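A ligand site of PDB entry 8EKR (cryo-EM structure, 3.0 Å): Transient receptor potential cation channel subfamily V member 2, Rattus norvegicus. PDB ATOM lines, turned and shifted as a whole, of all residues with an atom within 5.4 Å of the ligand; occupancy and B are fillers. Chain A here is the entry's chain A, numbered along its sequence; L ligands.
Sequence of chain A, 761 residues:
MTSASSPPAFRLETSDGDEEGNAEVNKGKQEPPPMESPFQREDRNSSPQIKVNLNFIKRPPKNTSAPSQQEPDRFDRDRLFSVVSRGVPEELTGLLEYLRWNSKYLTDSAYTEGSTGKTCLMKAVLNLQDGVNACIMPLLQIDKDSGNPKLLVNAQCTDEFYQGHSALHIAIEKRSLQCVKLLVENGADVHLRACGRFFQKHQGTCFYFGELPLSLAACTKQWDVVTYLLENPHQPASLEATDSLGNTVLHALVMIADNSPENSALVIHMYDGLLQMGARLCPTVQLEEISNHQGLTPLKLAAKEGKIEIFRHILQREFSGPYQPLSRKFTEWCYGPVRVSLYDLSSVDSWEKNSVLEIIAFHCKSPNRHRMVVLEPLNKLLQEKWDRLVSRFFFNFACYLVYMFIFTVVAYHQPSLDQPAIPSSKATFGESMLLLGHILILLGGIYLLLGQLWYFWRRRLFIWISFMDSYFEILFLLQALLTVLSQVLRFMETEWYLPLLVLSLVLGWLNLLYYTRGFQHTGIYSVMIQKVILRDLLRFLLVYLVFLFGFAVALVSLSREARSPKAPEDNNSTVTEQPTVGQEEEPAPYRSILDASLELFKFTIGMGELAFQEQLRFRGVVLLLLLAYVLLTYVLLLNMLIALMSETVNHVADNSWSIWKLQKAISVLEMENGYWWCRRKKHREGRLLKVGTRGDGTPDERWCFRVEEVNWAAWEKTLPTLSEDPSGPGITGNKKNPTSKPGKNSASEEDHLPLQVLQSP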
ATOM      1  N   PHE A 395       2.990  18.590  -9.497  1.00  0.00           N
ATOM      2  CA  PHE A 395       4.236  17.882  -9.234  1.00  0.00           C
ATOM      3  C   PHE A 395       5.438  18.637  -9.805  1.00  0.00           C
ATOM      4  O   PHE A 395       6.483  18.741  -9.148  1.00  0.00           O
ATOM      5  CB  PHE A 395       4.174  16.472  -9.812  1.00  0.00           C
ATOM      6  CG  PHE A 395       5.454  15.703  -9.684  1.00  0.00           C
ATOM      7  CD1 PHE A 395       5.875  15.251  -8.443  1.00  0.00           C
ATOM      8  CD2 PHE A 395       6.244  15.446 -10.789  1.00  0.00           C
ATOM      9  CE1 PHE A 395       7.054  14.535  -8.313  1.00  0.00           C
ATOM     10  CE2 PHE A 395       7.425  14.737 -10.666  1.00  0.00           C
ATOM     11  CZ  PHE A 395       7.833  14.289  -9.425  1.00  0.00           C
ATOM     12  N   ASN A 396       5.297  19.166 -11.029  1.00  0.00           N
ATOM     13  CA  ASN A 396       6.346  19.999 -11.604  1.00  0.00           C
ATOM     14  C   ASN A 396       6.550  21.273 -10.792  1.00  0.00           C
ATOM     15  O   ASN A 396       7.689  21.723 -10.599  1.00  0.00           O
ATOM     16  CB  ASN A 396       6.016  20.331 -13.057  1.00  0.00           C
ATOM     17  CG  ASN A 396       5.990  19.094 -13.942  1.00  0.00           C
ATOM     18  OD1 ASN A 396       6.047  17.970 -13.457  1.00  0.00           O
ATOM     19  ND2 ASN A 396       5.916  19.313 -15.242  1.00  0.00           N
ATOM     20  N   CYS A 399       8.527  20.248  -7.700  1.00  0.00           N
ATOM     21  CA  CYS A 399       9.927  19.990  -8.026  1.00  0.00           C
ATOM     22  C   CYS A 399      10.694  21.283  -8.269  1.00  0.00           C
ATOM     23  O   CYS A 399      11.822  21.441  -7.801  1.00  0.00           O
ATOM     24  CB  CYS A 399      10.016  19.083  -9.258  1.00  0.00           C
ATOM     25  SG  CYS A 399       9.539  17.374  -8.945  1.00  0.00           S
ATOM     26  N   TYR A 400      10.073  22.233  -8.972  1.00  0.00           N
ATOM     27  CA  TYR A 400      10.719  23.525  -9.203  1.00  0.00           C
ATOM     28  C   TYR A 400      10.886  24.313  -7.905  1.00  0.00           C
ATOM     29  O   TYR A 400      11.905  24.979  -7.704  1.00  0.00           O
ATOM     30  CB  TYR A 400       9.910  24.322 -10.225  1.00  0.00           C
ATOM     31  CG  TYR A 400      10.599  25.542 -10.775  1.00  0.00           C
ATOM     32  CD1 TYR A 400      11.632  25.416 -11.706  1.00  0.00           C
ATOM     33  CD2 TYR A 400      10.199  26.812 -10.413  1.00  0.00           C
ATOM     34  CE1 TYR A 400      12.259  26.526 -12.219  1.00  0.00           C
ATOM     35  CE2 TYR A 400      10.815  27.934 -10.933  1.00  0.00           C
ATOM     36  CZ  TYR A 400      11.846  27.780 -11.833  1.00  0.00           C
ATOM     37  OH  TYR A 400      12.467  28.896 -12.358  1.00  0.00           O
ATOM     38  N   VAL A 402      11.238  22.979  -4.859  1.00  0.00           N
ATOM     39  CA  VAL A 402      12.306  22.328  -4.114  1.00  0.00           C
ATOM     40  C   VAL A 402      13.671  22.709  -4.698  1.00  0.00           C
ATOM     41  O   VAL A 402      14.620  22.974  -3.960  1.00  0.00           O
ATOM     42  CB  VAL A 402      12.100  20.803  -4.092  1.00  0.00           C
ATOM     43  CG1 VAL A 402      13.349  20.074  -3.614  1.00  0.00           C
ATOM     44  CG2 VAL A 402      10.917  20.450  -3.192  1.00  0.00           C
ATOM     45  N   TYR A 403      13.760  22.748  -6.027  1.00  0.00           N
ATOM     46  CA  TYR A 403      15.007  23.109  -6.685  1.00  0.00           C
ATOM     47  C   TYR A 403      15.408  24.552  -6.354  1.00  0.00           C
ATOM     48  O   TYR A 403      16.576  24.833  -6.091  1.00  0.00           O
ATOM     49  CB  TYR A 403      14.882  22.906  -8.193  1.00  0.00           C
ATOM     50  CG  TYR A 403      15.920  23.625  -9.032  1.00  0.00           C
ATOM     51  CD1 TYR A 403      17.243  23.209  -9.033  1.00  0.00           C
ATOM     52  CD2 TYR A 403      15.553  24.696  -9.837  1.00  0.00           C
ATOM     53  CE1 TYR A 403      18.183  23.862  -9.816  1.00  0.00           C
ATOM     54  CE2 TYR A 403      16.490  25.342 -10.613  1.00  0.00           C
ATOM     55  CZ  TYR A 403      17.805  24.925 -10.603  1.00  0.00           C
ATOM     56  OH  TYR A 403      18.728  25.575 -11.379  1.00  0.00           O
ATOM     57  N   LEU A 443      23.194  19.969 -11.897  1.00  0.00           N
ATOM     58  CA  LEU A 443      22.330  18.966 -12.502  1.00  0.00           C
ATOM     59  C   LEU A 443      20.959  19.542 -12.859  1.00  0.00           C
ATOM     60  O   LEU A 443      20.439  19.285 -13.946  1.00  0.00           O
ATOM     61  CB  LEU A 443      22.171  17.767 -11.560  1.00  0.00           C
ATOM     62  CG  LEU A 443      23.406  16.868 -11.411  1.00  0.00           C
ATOM     63  CD1 LEU A 443      23.149  15.803 -10.357  1.00  0.00           C
ATOM     64  CD2 LEU A 443      23.781  16.241 -12.739  1.00  0.00           C
ATOM     65  N   GLY A 444      20.380  20.353 -11.961  1.00  0.00           N
ATOM     66  CA  GLY A 444      19.104  20.973 -12.258  1.00  0.00           C
ATOM     67  C   GLY A 444      19.191  21.971 -13.399  1.00  0.00           C
ATOM     68  O   GLY A 444      18.276  22.060 -14.238  1.00  0.00           O
ATOM     69  N   TYR A 447      19.457  19.991 -16.605  1.00  0.00           N
ATOM     70  CA  TYR A 447      18.144  19.420 -16.916  1.00  0.00           C
ATOM     71  C   TYR A 447      17.210  20.468 -17.510  1.00  0.00           C
ATOM     72  O   TYR A 447      16.544  20.224 -18.533  1.00  0.00           O
ATOM     73  CB  TYR A 447      17.547  18.816 -15.645  1.00  0.00           C
ATOM     74  CG  TYR A 447      16.237  18.088 -15.835  1.00  0.00           C
ATOM     75  CD1 TYR A 447      16.210  16.731 -16.161  1.00  0.00           C
ATOM     76  CD2 TYR A 447      15.019  18.732 -15.653  1.00  0.00           C
ATOM     77  CE1 TYR A 447      15.018  16.064 -16.326  1.00  0.00           C
ATOM     78  CE2 TYR A 447      13.821  18.071 -15.813  1.00  0.00           C
ATOM     79  CZ  TYR A 447      13.824  16.733 -16.152  1.00  0.00           C
ATOM     80  OH  TYR A 447      12.634  16.074 -16.307  1.00  0.00           O
ATOM     81  N   LEU A 448      17.163  21.650 -16.893  1.00  0.00           N
ATOM     82  CA  LEU A 448      16.304  22.727 -17.390  1.00  0.00           C
ATOM     83  C   LEU A 448      16.757  23.208 -18.768  1.00  0.00           C
ATOM     84  O   LEU A 448      15.935  23.478 -19.643  1.00  0.00           O
ATOM     85  CB  LEU A 448      16.276  23.881 -16.401  1.00  0.00           C
ATOM     86  CG  LEU A 448      15.356  23.724 -15.197  1.00  0.00           C
ATOM     87  CD1 LEU A 448      15.437  24.950 -14.300  1.00  0.00           C
ATOM     88  CD2 LEU A 448      13.925  23.475 -15.629  1.00  0.00           C
ATOM     89  N   GLN A 452      14.470  22.970 -22.117  1.00  0.00           N
ATOM     90  CA  GLN A 452      14.140  24.175 -22.861  1.00  0.00           C
ATOM     91  C   GLN A 452      14.672  24.105 -24.287  1.00  0.00           C
ATOM     92  O   GLN A 452      14.019  24.577 -25.222  1.00  0.00           O
ATOM     93  CB  GLN A 452      14.678  25.413 -22.139  1.00  0.00           C
ATOM     94  CG  GLN A 452      13.929  25.755 -20.872  1.00  0.00           C
ATOM     95  CD  GLN A 452      12.434  25.898 -21.100  1.00  0.00           C
ATOM     96  OE1 GLN A 452      12.003  26.694 -21.931  1.00  0.00           O
ATOM     97  NE2 GLN A 452      11.650  25.126 -20.373  1.00  0.00           N
ATOM     98  N   PHE A 472       8.027  33.078 -20.943  1.00  0.00           N
ATOM     99  CA  PHE A 472       8.501  32.365 -19.758  1.00  0.00           C
ATOM    100  C   PHE A 472       9.493  31.269 -20.099  1.00  0.00           C
ATOM    101  O   PHE A 472      10.523  31.155 -19.415  1.00  0.00           O
ATOM    102  CB  PHE A 472       7.351  31.751 -18.972  1.00  0.00           C
ATOM    103  CG  PHE A 472       6.595  32.720 -18.108  1.00  0.00           C
ATOM    104  CD1 PHE A 472       7.206  33.305 -17.016  1.00  0.00           C
ATOM    105  CD2 PHE A 472       5.272  33.009 -18.364  1.00  0.00           C
ATOM    106  CE1 PHE A 472       6.526  34.183 -16.209  1.00  0.00           C
ATOM    107  CE2 PHE A 472       4.570  33.890 -17.563  1.00  0.00           C
ATOM    108  CZ  PHE A 472       5.197  34.478 -16.477  1.00  0.00           C
ATOM    109  N   GLU A 473       9.219  30.493 -21.143  1.00  0.00           N
ATOM    110  CA  GLU A 473      10.170  29.488 -21.617  1.00  0.00           C
ATOM    111  C   GLU A 473      11.508  30.134 -21.954  1.00  0.00           C
ATOM    112  O   GLU A 473      12.559  29.605 -21.583  1.00  0.00           O
ATOM    113  CB  GLU A 473       9.599  28.750 -22.838  1.00  0.00           C
ATOM    114  CG  GLU A 473       8.439  27.819 -22.533  1.00  0.00           C
ATOM    115  CD  GLU A 473       7.098  28.528 -22.517  1.00  0.00           C
ATOM    116  OE1 GLU A 473       7.070  29.751 -22.812  1.00  0.00           O
ATOM    117  OE2 GLU A 473       6.080  27.877 -22.210  1.00  0.00           O
ATOM    118  N   PHE A 476      12.833  30.712 -18.825  1.00  0.00           N
ATOM    119  CA  PHE A 476      13.213  29.399 -18.310  1.00  0.00           C
ATOM    120  C   PHE A 476      14.447  28.873 -19.016  1.00  0.00           C
ATOM    121  O   PHE A 476      15.140  28.013 -18.481  1.00  0.00           O
ATOM    122  CB  PHE A 476      12.053  28.415 -18.447  1.00  0.00           C
ATOM    123  CG  PHE A 476      11.226  28.271 -17.203  1.00  0.00           C
ATOM    124  CD1 PHE A 476      10.318  29.239 -16.848  1.00  0.00           C
ATOM    125  CD2 PHE A 476      11.385  27.161 -16.390  1.00  0.00           C
ATOM    126  CE1 PHE A 476       9.558  29.108 -15.703  1.00  0.00           C
ATOM    127  CE2 PHE A 476      10.628  27.016 -15.244  1.00  0.00           C
ATOM    128  CZ  PHE A 476       9.709  27.996 -14.895  1.00  0.00           C
ATOM    129  N   TYR A 514       4.958  31.568 -13.376  1.00  0.00           N
ATOM    130  CA  TYR A 514       4.348  30.748 -14.423  1.00  0.00           C
ATOM    131  C   TYR A 514       3.266  29.845 -13.831  1.00  0.00           C
ATOM    132  O   TYR A 514       2.135  29.807 -14.336  1.00  0.00           O
ATOM    133  CB  TYR A 514       5.424  29.918 -15.118  1.00  0.00           C
ATOM    134  CG  TYR A 514       4.904  28.770 -15.951  1.00  0.00           C
ATOM    135  CD1 TYR A 514       4.373  28.989 -17.221  1.00  0.00           C
ATOM    136  CD2 TYR A 514       4.967  27.465 -15.482  1.00  0.00           C
ATOM    137  CE1 TYR A 514       3.907  27.936 -17.986  1.00  0.00           C
ATOM    138  CE2 TYR A 514       4.493  26.411 -16.235  1.00  0.00           C
ATOM    139  CZ  TYR A 514       3.967  26.647 -17.483  1.00  0.00           C
ATOM    140  OH  TYR A 514       3.496  25.600 -18.242  1.00  0.00           O
ATOM    141  N   TYR A 515       3.580  29.160 -12.729  1.00  0.00           N
ATOM    142  CA  TYR A 515       2.662  28.210 -12.123  1.00  0.00           C
ATOM    143  C   TYR A 515       1.428  28.880 -11.520  1.00  0.00           C
ATOM    144  O   TYR A 515       0.466  28.177 -11.185  1.00  0.00           O
ATOM    145  CB  TYR A 515       3.396  27.394 -11.059  1.00  0.00           C
ATOM    146  CG  TYR A 515       4.595  26.649 -11.604  1.00  0.00           C
ATOM    147  CD1 TYR A 515       4.434  25.406 -12.204  1.00  0.00           C
ATOM    148  CD2 TYR A 515       5.870  27.182 -11.528  1.00  0.00           C
ATOM    149  CE1 TYR A 515       5.519  24.720 -12.713  1.00  0.00           C
ATOM    150  CE2 TYR A 515       6.962  26.499 -12.030  1.00  0.00           C
ATOM    151  CZ  TYR A 515       6.777  25.273 -12.621  1.00  0.00           C
ATOM    152  OH  TYR A 515       7.856  24.594 -13.124  1.00  0.00           O
ATOM    153  N   TYR A 675       8.208  14.497 -20.599  1.00  0.00           N
ATOM    154  CA  TYR A 675       9.502  15.134 -20.444  1.00  0.00           C
ATOM    155  C   TYR A 675      10.395  14.782 -21.630  1.00  0.00           C
ATOM    156  O   TYR A 675      10.034  14.000 -22.511  1.00  0.00           O
ATOM    157  CB  TYR A 675      10.129  14.720 -19.119  1.00  0.00           C
ATOM    158  CG  TYR A 675       9.201  14.842 -17.928  1.00  0.00           C
ATOM    159  CD1 TYR A 675       8.792  16.094 -17.478  1.00  0.00           C
ATOM    160  CD2 TYR A 675       8.737  13.716 -17.269  1.00  0.00           C
ATOM    161  CE1 TYR A 675       7.938  16.208 -16.391  1.00  0.00           C
ATOM    162  CE2 TYR A 675       7.888  13.823 -16.187  1.00  0.00           C
ATOM    163  CZ  TYR A 675       7.488  15.076 -15.748  1.00  0.00           C
ATOM    164  OH  TYR A 675       6.642  15.191 -14.673  1.00  0.00           O
ATOM    165  N   TRP A 677      13.213  13.159 -21.443  1.00  0.00           N
ATOM    166  CA  TRP A 677      13.871  11.871 -21.243  1.00  0.00           C
ATOM    167  C   TRP A 677      12.925  10.685 -21.349  1.00  0.00           C
ATOM    168  O   TRP A 677      13.368   9.584 -21.688  1.00  0.00           O
ATOM    169  CB  TRP A 677      14.594  11.868 -19.895  1.00  0.00           C
ATOM    170  CG  TRP A 677      13.708  12.112 -18.719  1.00  0.00           C
ATOM    171  CD1 TRP A 677      13.303  13.330 -18.243  1.00  0.00           C
ATOM    172  CD2 TRP A 677      13.140  11.133 -17.838  1.00  0.00           C
ATOM    173  NE1 TRP A 677      12.497  13.151 -17.141  1.00  0.00           N
ATOM    174  CE2 TRP A 677      12.391  11.822 -16.868  1.00  0.00           C
ATOM    175  CE3 TRP A 677      13.186   9.730 -17.791  1.00  0.00           C
ATOM    176  CZ2 TRP A 677      11.692  11.166 -15.859  1.00  0.00           C
ATOM    177  CZ3 TRP A 677      12.498   9.084 -16.784  1.00  0.00           C
ATOM    178  CH2 TRP A 677      11.756   9.794 -15.832  1.00  0.00           C
HETATM  179  O1  LIG L   1       7.182  22.680 -15.795  1.00  0.00           O
HETATM  180  O2  LIG L   1       8.174  21.234 -17.523  1.00  0.00           O
HETATM  181  P1  LIG L   1       8.435  22.377 -16.568  1.00  0.00           P
HETATM  182  O3  LIG L   1       9.628  21.937 -15.525  1.00  0.00           O
HETATM  183  C1  LIG L   1       9.282  21.675 -14.198  1.00  0.00           C
HETATM  184  C2  LIG L   1      10.259  20.688 -13.580  1.00  0.00           C
HETATM  185  C3  LIG L   1      10.074  19.307 -14.223  1.00  0.00           C
HETATM  186  O4  LIG L   1      11.199  18.531 -13.978  1.00  0.00           O
HETATM  187  C4  LIG L   1      10.960  17.393 -13.191  1.00  0.00           C
HETATM  188  O5  LIG L   1       9.865  17.005 -13.023  1.00  0.00           O
HETATM  189  C5  LIG L   1      12.142  16.656 -12.544  1.00  0.00           C
HETATM  190  C6  LIG L   1      12.225  15.233 -13.092  1.00  0.00           C
HETATM  191  C7  LIG L   1      12.950  14.347 -12.081  1.00  0.00           C
HETATM  192  C8  LIG L   1      14.457  14.355 -12.402  1.00  0.00           C
HETATM  193  C9  LIG L   1      14.750  13.290 -13.461  1.00  0.00           C
HETATM  194  C10 LIG L   1      16.249  13.256 -13.756  1.00  0.00           C
HETATM  195  C11 LIG L   1      17.015  12.873 -12.480  1.00  0.00           C
HETATM  196  C12 LIG L   1      18.503  12.784 -12.794  1.00  0.00           C
HETATM  197  C13 LIG L   1      19.288  12.630 -11.499  1.00  0.00           C
HETATM  198  O6  LIG L   1      11.576  21.129 -13.798  1.00  0.00           O
HETATM  199  C14 LIG L   1      12.334  21.235 -12.626  1.00  0.00           C
HETATM  200  O7  LIG L   1      11.809  21.409 -11.584  1.00  0.00           O
HETATM  201  C15 LIG L   1      13.860  21.120 -12.701  1.00  0.00           C
HETATM  202  C16 LIG L   1      14.378  20.674 -11.333  1.00  0.00           C
HETATM  203  C17 LIG L   1      15.519  19.675 -11.530  1.00  0.00           C
HETATM  204  C18 LIG L   1      15.764  18.912 -10.232  1.00  0.00           C
HETATM  205  C19 LIG L   1      14.508  18.118  -9.856  1.00  0.00           C
HETATM  206  C20 LIG L   1      14.556  17.770  -8.367  1.00  0.00           C
HETATM  207  C21 LIG L   1      13.332  16.916  -8.015  1.00  0.00           C
HETATM  208  C22 LIG L   1      13.182  16.843  -6.499  1.00  0.00           C
HETATM  209  C23 LIG L   1      12.044  15.890  -6.146  1.00  0.00           C
HETATM  210  O8  LIG L   1       8.898  23.706 -17.421  1.00  0.00           O
HETATM  211  C24 LIG L   1       7.955  24.706 -17.647  1.00  0.00           C
HETATM  212  C25 LIG L   1       8.603  25.861 -18.401  1.00  0.00           C
HETATM  213  N1  LIG L   1       7.570  26.760 -18.891  1.00  0.00           N
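O7 of the ligand sits at hydrogen-bond distance from N of Tyr 400 (3.2 Å). OH of Tyr 515 is in hydrogen-bond range of O1 of the ligand, at 3.4 Å. The side-chain carboxylate (OE2) of Glu 473 lies within salt-bridge range of a nitrogen (N1) of the ligand (3.8 Å).
The side-chain hydroxyl (OH) of Tyr 447 is in hydrogen-bond range of the indole nitrogen (NE1) of Trp 677, 3.0 Å away. O of Phe 395 is in hydrogen-bond range of SG of Cys 399 (3.4 Å). The side-chain hydroxyl (OH) of Tyr 675 is in hydrogen-bond range of the side-chain amide oxygen (OD1) of Asn 396. The backbone carbonyl oxygen (O) of Glu 473 sits close to the side-chain amide oxygen (OE1) of Gln 452, 3.0 Å away.
Residues that only touch the ligand: Tyr 447 (3.2 Å), Cys 399 (3.5 Å), Asn 396 (3.6 Å), Phe 476 (3.7 Å), Gln 452 (3.7 Å), Leu 448 (3.8 Å), Tyr 514 (3.9 Å), Gly 444 (3.9 Å), Tyr 403 (3.9 Å) and Tyr 675 (3.96 Å). Hydrophobic or aromatic side chains within 4 Å of the ligand: Tyr 400, Tyr 403, Tyr 447, Leu 448, Phe 476, Tyr 514 and Tyr 675. Along chain A the residues within 4 Å of the ligand span positions 396 to 675.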
